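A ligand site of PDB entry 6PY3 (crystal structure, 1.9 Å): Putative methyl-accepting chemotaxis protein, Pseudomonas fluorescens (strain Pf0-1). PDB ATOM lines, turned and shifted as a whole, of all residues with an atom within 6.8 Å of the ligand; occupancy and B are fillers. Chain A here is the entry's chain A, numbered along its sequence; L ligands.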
ATOM      1  N   ALA A  72     -13.776 -23.466  -5.157  1.00  0.00           N
ATOM      2  CA  ALA A  72     -13.567 -23.343  -6.575  1.00  0.00           C
ATOM      3  C   ALA A  72     -14.644 -22.412  -7.140  1.00  0.00           C
ATOM      4  O   ALA A  72     -15.674 -22.130  -6.489  1.00  0.00           O
ATOM      5  CB  ALA A  72     -13.681 -24.712  -7.255  1.00  0.00           C
ATOM      6  N   SER A  73     -14.281 -21.793  -8.258  1.00  0.00           N
ATOM      7  CA  SER A  73     -15.235 -21.122  -9.099  1.00  0.00           C
ATOM      8  C   SER A  73     -15.211 -21.648 -10.515  1.00  0.00           C
ATOM      9  O   SER A  73     -14.243 -22.275 -10.987  1.00  0.00           O
ATOM     10  CB  SER A  73     -14.978 -19.606  -9.145  1.00  0.00           C
ATOM     11  OG  SER A  73     -13.694 -19.334  -9.666  1.00  0.00           O
ATOM     12  N   TYR A  74     -16.263 -21.334 -11.243  1.00  0.00           N
ATOM     13  CA  TYR A  74     -16.519 -22.025 -12.485  1.00  0.00           C
ATOM     14  C   TYR A  74     -17.535 -21.223 -13.279  1.00  0.00           C
ATOM     15  O   TYR A  74     -18.359 -20.470 -12.728  1.00  0.00           O
ATOM     16  CB  TYR A  74     -17.108 -23.434 -12.177  1.00  0.00           C
ATOM     17  CG  TYR A  74     -18.070 -23.461 -11.018  1.00  0.00           C
ATOM     18  CD1 TYR A  74     -19.422 -23.286 -11.229  1.00  0.00           C
ATOM     19  CD2 TYR A  74     -17.672 -23.823  -9.755  1.00  0.00           C
ATOM     20  CE1 TYR A  74     -20.311 -23.235 -10.177  1.00  0.00           C
ATOM     21  CE2 TYR A  74     -18.550 -23.816  -8.711  1.00  0.00           C
ATOM     22  CZ  TYR A  74     -19.870 -23.516  -8.932  1.00  0.00           C
ATOM     23  OH  TYR A  74     -20.779 -23.564  -7.912  1.00  0.00           O
ATOM     24  N   LEU A  75     -17.558 -21.551 -14.572  1.00  0.00           N
ATOM     25  CA  LEU A  75     -18.538 -21.089 -15.531  1.00  0.00           C
ATOM     26  C   LEU A  75     -19.091 -22.326 -16.224  1.00  0.00           C
ATOM     27  O   LEU A  75     -18.309 -23.189 -16.659  1.00  0.00           O
ATOM     28  CB  LEU A  75     -17.860 -20.228 -16.599  1.00  0.00           C
ATOM     29  CG  LEU A  75     -18.758 -19.818 -17.779  1.00  0.00           C
ATOM     30  CD1 LEU A  75     -19.946 -18.974 -17.370  1.00  0.00           C
ATOM     31  CD2 LEU A  75     -17.936 -19.061 -18.820  1.00  0.00           C
ATOM     32  N   PHE A  82     -18.093 -26.615 -19.266  1.00  0.00           N
ATOM     33  CA  PHE A  82     -17.791 -25.839 -18.049  1.00  0.00           C
ATOM     34  C   PHE A  82     -16.289 -25.676 -17.896  1.00  0.00           C
ATOM     35  O   PHE A  82     -15.519 -26.365 -18.554  1.00  0.00           O
ATOM     36  CB  PHE A  82     -18.350 -26.516 -16.802  1.00  0.00           C
ATOM     37  CG  PHE A  82     -17.739 -27.851 -16.509  1.00  0.00           C
ATOM     38  CD1 PHE A  82     -18.224 -29.014 -17.106  1.00  0.00           C
ATOM     39  CD2 PHE A  82     -16.603 -27.952 -15.733  1.00  0.00           C
ATOM     40  CE1 PHE A  82     -17.664 -30.249 -16.829  1.00  0.00           C
ATOM     41  CE2 PHE A  82     -16.012 -29.179 -15.473  1.00  0.00           C
ATOM     42  CZ  PHE A  82     -16.535 -30.322 -16.040  1.00  0.00           C
ATOM     43  N   THR A  83     -15.897 -24.689 -17.096  1.00  0.00           N
ATOM     44  CA  THR A  83     -14.518 -24.480 -16.670  1.00  0.00           C
ATOM     45  C   THR A  83     -14.519 -24.277 -15.170  1.00  0.00           C
ATOM     46  O   THR A  83     -15.302 -23.469 -14.652  1.00  0.00           O
ATOM     47  CB  THR A  83     -13.908 -23.225 -17.309  1.00  0.00           C
ATOM     48  OG1 THR A  83     -13.700 -23.458 -18.702  1.00  0.00           O
ATOM     49  CG2 THR A  83     -12.558 -22.870 -16.665  1.00  0.00           C
ATOM     50  N   ILE A  84     -13.626 -24.988 -14.477  1.00  0.00           N
ATOM     51  CA  ILE A  84     -13.568 -24.900 -13.029  1.00  0.00           C
ATOM     52  C   ILE A  84     -12.128 -24.645 -12.644  1.00  0.00           C
ATOM     53  O   ILE A  84     -11.191 -25.121 -13.300  1.00  0.00           O
ATOM     54  CB  ILE A  84     -14.140 -26.162 -12.348  1.00  0.00           C
ATOM     55  CG1 ILE A  84     -14.090 -26.052 -10.825  1.00  0.00           C
ATOM     56  CG2 ILE A  84     -13.455 -27.430 -12.815  1.00  0.00           C
ATOM     57  CD1 ILE A  84     -14.677 -27.230 -10.087  1.00  0.00           C
ATOM     58  N   MET A  90     -13.937 -34.376 -12.593  1.00  0.00           N
ATOM     59  CA  MET A  90     -15.379 -34.432 -12.374  1.00  0.00           C
ATOM     60  C   MET A  90     -15.936 -35.835 -12.602  1.00  0.00           C
ATOM     61  O   MET A  90     -15.349 -36.640 -13.315  1.00  0.00           O
ATOM     62  CB  MET A  90     -16.084 -33.392 -13.241  1.00  0.00           C
ATOM     63  CG  MET A  90     -15.623 -31.970 -12.975  1.00  0.00           C
ATOM     64  SD  MET A  90     -15.823 -31.426 -11.255  1.00  0.00           S
ATOM     65  CE  MET A  90     -17.581 -31.459 -11.155  1.00  0.00           C
ATOM     66  N   PHE A  94     -20.887 -35.861 -15.663  1.00  0.00           N
ATOM     67  CA  PHE A  94     -21.185 -34.549 -15.061  1.00  0.00           C
ATOM     68  C   PHE A  94     -21.681 -33.528 -16.071  1.00  0.00           C
ATOM     69  O   PHE A  94     -21.062 -33.306 -17.114  1.00  0.00           O
ATOM     70  CB  PHE A  94     -19.964 -33.952 -14.364  1.00  0.00           C
ATOM     71  CG  PHE A  94     -20.227 -32.593 -13.818  1.00  0.00           C
ATOM     72  CD1 PHE A  94     -20.943 -32.450 -12.640  1.00  0.00           C
ATOM     73  CD2 PHE A  94     -19.749 -31.460 -14.475  1.00  0.00           C
ATOM     74  CE1 PHE A  94     -21.227 -31.184 -12.151  1.00  0.00           C
ATOM     75  CE2 PHE A  94     -19.950 -30.203 -13.947  1.00  0.00           C
ATOM     76  CZ  PHE A  94     -20.704 -30.073 -12.798  1.00  0.00           C
ATOM     77  N   ASP A  95     -22.802 -32.884 -15.750  1.00  0.00           N
ATOM     78  CA  ASP A  95     -23.415 -31.864 -16.617  1.00  0.00           C
ATOM     79  C   ASP A  95     -23.767 -30.657 -15.760  1.00  0.00           C
ATOM     80  O   ASP A  95     -24.699 -30.738 -14.994  1.00  0.00           O
ATOM     81  CB  ASP A  95     -24.690 -32.427 -17.284  1.00  0.00           C
ATOM     82  CG  ASP A  95     -25.316 -31.482 -18.308  1.00  0.00           C
ATOM     83  OD1 ASP A  95     -24.878 -30.294 -18.447  1.00  0.00           O
ATOM     84  OD2 ASP A  95     -26.249 -31.931 -19.030  1.00  0.00           O
ATOM     85  N   PRO A  96     -23.154 -29.480 -16.031  1.00  0.00           N
ATOM     86  CA  PRO A  96     -23.398 -28.323 -15.186  1.00  0.00           C
ATOM     87  C   PRO A  96     -24.826 -27.805 -15.213  1.00  0.00           C
ATOM     88  O   PRO A  96     -25.352 -27.317 -14.197  1.00  0.00           O
ATOM     89  CB  PRO A  96     -22.438 -27.268 -15.772  1.00  0.00           C
ATOM     90  CG  PRO A  96     -22.096 -27.745 -17.140  1.00  0.00           C
ATOM     91  CD  PRO A  96     -22.091 -29.234 -17.025  1.00  0.00           C
ATOM     92  N   ARG A  99     -27.275 -28.891 -12.422  1.00  0.00           N
ATOM     93  CA  ARG A  99     -26.791 -28.693 -11.050  1.00  0.00           C
ATOM     94  C   ARG A  99     -27.530 -27.538 -10.371  1.00  0.00           C
ATOM     95  O   ARG A  99     -28.000 -26.624 -11.044  1.00  0.00           O
ATOM     96  CB  ARG A  99     -25.292 -28.408 -11.095  1.00  0.00           C
ATOM     97  CG  ARG A  99     -24.467 -29.511 -11.720  1.00  0.00           C
ATOM     98  CD  ARG A  99     -24.542 -30.815 -10.950  1.00  0.00           C
ATOM     99  NE  ARG A  99     -23.810 -30.730  -9.695  1.00  0.00           N
ATOM    100  CZ  ARG A  99     -23.976 -31.552  -8.661  1.00  0.00           C
ATOM    101  NH1 ARG A  99     -24.881 -32.523  -8.732  1.00  0.00           N
ATOM    102  NH2 ARG A  99     -23.248 -31.407  -7.566  1.00  0.00           N
ATOM    103  N   PRO A 100     -27.659 -27.566  -9.032  1.00  0.00           N
ATOM    104  CA  PRO A 100     -28.561 -26.585  -8.395  1.00  0.00           C
ATOM    105  C   PRO A 100     -28.116 -25.112  -8.547  1.00  0.00           C
ATOM    106  O   PRO A 100     -28.937 -24.203  -8.624  1.00  0.00           O
ATOM    107  CB  PRO A 100     -28.610 -27.012  -6.922  1.00  0.00           C
ATOM    108  CG  PRO A 100     -27.529 -28.000  -6.741  1.00  0.00           C
ATOM    109  CD  PRO A 100     -27.116 -28.547  -8.088  1.00  0.00           C
ATOM    110  N   TRP A 101     -26.813 -24.874  -8.676  1.00  0.00           N
ATOM    111  CA  TRP A 101     -26.319 -23.508  -8.908  1.00  0.00           C
ATOM    112  C   TRP A 101     -26.755 -22.970 -10.250  1.00  0.00           C
ATOM    113  O   TRP A 101     -27.046 -21.785 -10.360  1.00  0.00           O
ATOM    114  CB  TRP A 101     -24.795 -23.432  -8.771  1.00  0.00           C
ATOM    115  CG  TRP A 101     -23.989 -24.412  -9.576  1.00  0.00           C
ATOM    116  CD1 TRP A 101     -23.575 -25.652  -9.201  1.00  0.00           C
ATOM    117  CD2 TRP A 101     -23.539 -24.236 -10.908  1.00  0.00           C
ATOM    118  NE1 TRP A 101     -22.952 -26.272 -10.232  1.00  0.00           N
ATOM    119  CE2 TRP A 101     -22.850 -25.381 -11.271  1.00  0.00           C
ATOM    120  CE3 TRP A 101     -23.539 -23.143 -11.785  1.00  0.00           C
ATOM    121  CZ2 TRP A 101     -22.238 -25.526 -12.506  1.00  0.00           C
ATOM    122  CZ3 TRP A 101     -22.913 -23.270 -12.976  1.00  0.00           C
ATOM    123  CH2 TRP A 101     -22.214 -24.421 -13.311  1.00  0.00           C
ATOM    124  N   TYR A 117     -26.006 -28.636  -0.834  1.00  0.00           N
ATOM    125  CA  TYR A 117     -26.039 -29.789  -1.738  1.00  0.00           C
ATOM    126  C   TYR A 117     -24.667 -30.471  -1.765  1.00  0.00           C
ATOM    127  O   TYR A 117     -23.681 -29.918  -1.261  1.00  0.00           O
ATOM    128  CB  TYR A 117     -26.460 -29.327  -3.132  1.00  0.00           C
ATOM    129  CG  TYR A 117     -25.420 -28.530  -3.900  1.00  0.00           C
ATOM    130  CD1 TYR A 117     -25.252 -27.173  -3.678  1.00  0.00           C
ATOM    131  CD2 TYR A 117     -24.659 -29.106  -4.907  1.00  0.00           C
ATOM    132  CE1 TYR A 117     -24.381 -26.429  -4.454  1.00  0.00           C
ATOM    133  CE2 TYR A 117     -23.764 -28.379  -5.642  1.00  0.00           C
ATOM    134  CZ  TYR A 117     -23.593 -27.030  -5.372  1.00  0.00           C
ATOM    135  OH  TYR A 117     -22.699 -26.320  -6.118  1.00  0.00           O
ATOM    136  N   ILE A 118     -24.586 -31.640  -2.408  1.00  0.00           N
ATOM    137  CA  ILE A 118     -23.334 -32.396  -2.508  1.00  0.00           C
ATOM    138  C   ILE A 118     -22.441 -31.999  -3.669  1.00  0.00           C
ATOM    139  O   ILE A 118     -22.758 -32.138  -4.862  1.00  0.00           O
ATOM    140  CB  ILE A 118     -23.572 -33.929  -2.565  1.00  0.00           C
ATOM    141  CG1 ILE A 118     -24.589 -34.350  -1.513  1.00  0.00           C
ATOM    142  CG2 ILE A 118     -22.241 -34.647  -2.442  1.00  0.00           C
ATOM    143  CD1 ILE A 118     -25.036 -35.806  -1.532  1.00  0.00           C
ATOM    144  N   ASP A 119     -21.257 -31.495  -3.334  1.00  0.00           N
ATOM    145  CA  ASP A 119     -20.358 -30.975  -4.337  1.00  0.00           C
ATOM    146  C   ASP A 119     -19.905 -32.105  -5.286  1.00  0.00           C
ATOM    147  O   ASP A 119     -19.531 -33.183  -4.806  1.00  0.00           O
ATOM    148  CB  ASP A 119     -19.156 -30.348  -3.593  1.00  0.00           C
ATOM    149  CG  ASP A 119     -18.123 -29.753  -4.528  1.00  0.00           C
ATOM    150  OD1 ASP A 119     -18.447 -29.481  -5.703  1.00  0.00           O
ATOM    151  OD2 ASP A 119     -16.971 -29.560  -4.067  1.00  0.00           O
ATOM    152  N   ALA A 120     -20.053 -31.906  -6.592  1.00  0.00           N
ATOM    153  CA  ALA A 120     -19.573 -32.905  -7.560  1.00  0.00           C
ATOM    154  C   ALA A 120     -18.067 -33.074  -7.469  1.00  0.00           C
ATOM    155  O   ALA A 120     -17.547 -34.178  -7.690  1.00  0.00           O
ATOM    156  CB  ALA A 120     -19.986 -32.556  -8.982  1.00  0.00           C
ATOM    157  N   ALA A 121     -17.355 -31.958  -7.283  1.00  0.00           N
ATOM    158  CA  ALA A 121     -15.900 -31.987  -7.106  1.00  0.00           C
ATOM    159  C   ALA A 121     -15.366 -32.701  -5.858  1.00  0.00           C
ATOM    160  O   ALA A 121     -14.483 -33.557  -5.974  1.00  0.00           O
ATOM    161  CB  ALA A 121     -15.329 -30.571  -7.225  1.00  0.00           C
ATOM    162  N   THR A 122     -15.791 -32.299  -4.672  1.00  0.00           N
ATOM    163  CA  THR A 122     -15.224 -32.801  -3.418  1.00  0.00           C
ATOM    164  C   THR A 122     -16.033 -33.894  -2.760  1.00  0.00           C
ATOM    165  O   THR A 122     -15.540 -34.548  -1.848  1.00  0.00           O
ATOM    166  CB  THR A 122     -15.032 -31.668  -2.415  1.00  0.00           C
ATOM    167  OG1 THR A 122     -16.310 -31.154  -1.987  1.00  0.00           O
ATOM    168  CG2 THR A 122     -14.164 -30.526  -3.010  1.00  0.00           C
ATOM    169  N   ILE A 126     -21.898 -28.351   0.527  1.00  0.00           N
ATOM    170  CA  ILE A 126     -21.468 -26.994   0.281  1.00  0.00           C
ATOM    171  C   ILE A 126     -22.705 -26.154   0.000  1.00  0.00           C
ATOM    172  O   ILE A 126     -23.813 -26.678  -0.189  1.00  0.00           O
ATOM    173  CB  ILE A 126     -20.505 -26.888  -0.906  1.00  0.00           C
ATOM    174  CG1 ILE A 126     -21.181 -27.369  -2.208  1.00  0.00           C
ATOM    175  CG2 ILE A 126     -19.247 -27.757  -0.710  1.00  0.00           C
ATOM    176  CD1 ILE A 126     -20.400 -27.036  -3.457  1.00  0.00           C
ATOM    177  N   ILE A 127     -22.481 -24.863  -0.192  1.00  0.00           N
ATOM    178  CA  ILE A 127     -23.475 -24.048  -0.848  1.00  0.00           C
ATOM    179  C   ILE A 127     -22.759 -23.297  -1.938  1.00  0.00           C
ATOM    180  O   ILE A 127     -21.516 -23.332  -2.049  1.00  0.00           O
ATOM    181  CB  ILE A 127     -24.218 -23.048   0.082  1.00  0.00           C
ATOM    182  CG1 ILE A 127     -23.282 -21.979   0.632  1.00  0.00           C
ATOM    183  CG2 ILE A 127     -24.935 -23.750   1.188  1.00  0.00           C
ATOM    184  CD1 ILE A 127     -23.999 -20.774   1.198  1.00  0.00           C
ATOM    185  N   SER A 128     -23.537 -22.680  -2.794  1.00  0.00           N
ATOM    186  CA  SER A 128     -22.919 -21.943  -3.868  1.00  0.00           C
ATOM    187  C   SER A 128     -23.580 -20.599  -4.041  1.00  0.00           C
ATOM    188  O   SER A 128     -24.779 -20.472  -3.876  1.00  0.00           O
ATOM    189  CB  SER A 128     -23.013 -22.751  -5.173  1.00  0.00           C
ATOM    190  OG  SER A 128     -22.147 -23.867  -5.097  1.00  0.00           O
ATOM    191  N   GLY A 145     -19.484 -19.984  -7.267  1.00  0.00           N
ATOM    192  CA  GLY A 145     -18.411 -20.203  -6.287  1.00  0.00           C
ATOM    193  C   GLY A 145     -18.884 -21.011  -5.089  1.00  0.00           C
ATOM    194  O   GLY A 145     -19.987 -20.824  -4.574  1.00  0.00           O
ATOM    195  N   ASP A 146     -18.038 -21.896  -4.581  1.00  0.00           N
ATOM    196  CA  ASP A 146     -18.469 -22.861  -3.587  1.00  0.00           C
ATOM    197  C   ASP A 146     -17.871 -22.494  -2.230  1.00  0.00           C
ATOM    198  O   ASP A 146     -16.689 -22.124  -2.109  1.00  0.00           O
ATOM    199  CB  ASP A 146     -17.994 -24.262  -3.953  1.00  0.00           C
ATOM    200  CG  ASP A 146     -18.555 -24.752  -5.275  1.00  0.00           C
ATOM    201  OD1 ASP A 146     -19.696 -24.351  -5.634  1.00  0.00           O
ATOM    202  OD2 ASP A 146     -17.861 -25.609  -5.870  1.00  0.00           O
HETATM  203  N1  LIG L   1     -19.766 -27.319  -6.958  1.00  0.00           N
HETATM  204  C1  LIG L   1     -20.214 -27.388  -8.347  1.00  0.00           C
HETATM  205  C2  LIG L   1     -21.146 -28.610  -8.472  1.00  0.00           C
HETATM  206  O1  LIG L   1     -21.902 -28.738  -9.443  1.00  0.00           O
HETATM  207  C3  LIG L   1     -19.015 -27.449  -9.315  1.00  0.00           C
HETATM  208  C4  LIG L   1     -19.415 -27.177 -10.751  1.00  0.00           C
HETATM  209  C5  LIG L   1     -18.326 -28.797  -9.194  1.00  0.00           C
HETATM  210  C6  LIG L   1     -18.288 -27.095 -11.760  1.00  0.00           C
HETATM  211  O2  LIG L   1     -21.152 -29.498  -7.613  1.00  0.00           O
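NE of Arg 99 lies within salt-bridge range of O1 of the ligand, at 2.8 Å.
N1 of the ligand is in salt-bridge range of OD2 of Asp 146, 2.8 Å away.
The indole nitrogen (NE1) of Trp 101 sits at hydrogen-bond distance from an oxygen (O1) of the ligand (2.8 Å).
A nitrogen (N1) of the ligand is in salt-bridge range of the side-chain carboxylate (OD1) of Asp 119 (2.8 Å).
The backbone NH (N) of Ala 120 sits at hydrogen-bond distance from an oxygen (O2) of the ligand (2.8 Å).
The side-chain hydroxyl of Tyr 117 is in hydrogen-bond range of a nitrogen (N1) of the ligand (3.2 Å).
O of Ile 118 sits at hydrogen-bond distance from NH2 of Arg 99 (2.8 Å).
The side-chain carboxylate (OD1) of Asp 146 is in hydrogen-bond range of the side-chain hydroxyl (OH) of Tyr 74 (2.6 Å).
The side-chain carboxylate of Asp 146 lies within hydrogen-bond range of the side-chain hydroxyl of Ser 128, at 2.6 Å.
The backbone NH (N) of Asp 146 sits at hydrogen-bond distance from the backbone carbonyl oxygen (O) of Ala 72, 3.0 Å away.
OG1 of Thr 122 lies within hydrogen-bond range of OD2 of Asp 119 (2.7 Å).
The backbone NH of Ile 126 lies within hydrogen-bond range of the backbone carbonyl oxygen of Tyr 117, 3.0 Å away.
The side-chain hydroxyl of Ser 128 lies within hydrogen-bond range of the side-chain hydroxyl of Tyr 117, 2.7 Å away.
The side-chain hydroxyl of Tyr 74 is in hydrogen-bond range of the side-chain hydroxyl of Ser 128, at 3.1 Å.
Merely in contact with the ligand: Met 90, Ile 126, Phe 94, Tyr 74, Ala 121 and Ile 84.
Hydrophobic or aromatic side chains that line the ligand: Tyr 74, Ile 84, Met 90, Phe 94, Trp 101, Tyr 117, Ala 120 and Ile 126.
Of the 25 residues printed, 12 come within 4 Å of the ligand.
Along chain A the residues within 4 Å of the ligand span positions 74 to 146.
The nearest printed residue that does not touch the ligand is Ile 118 (4.1 Å).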
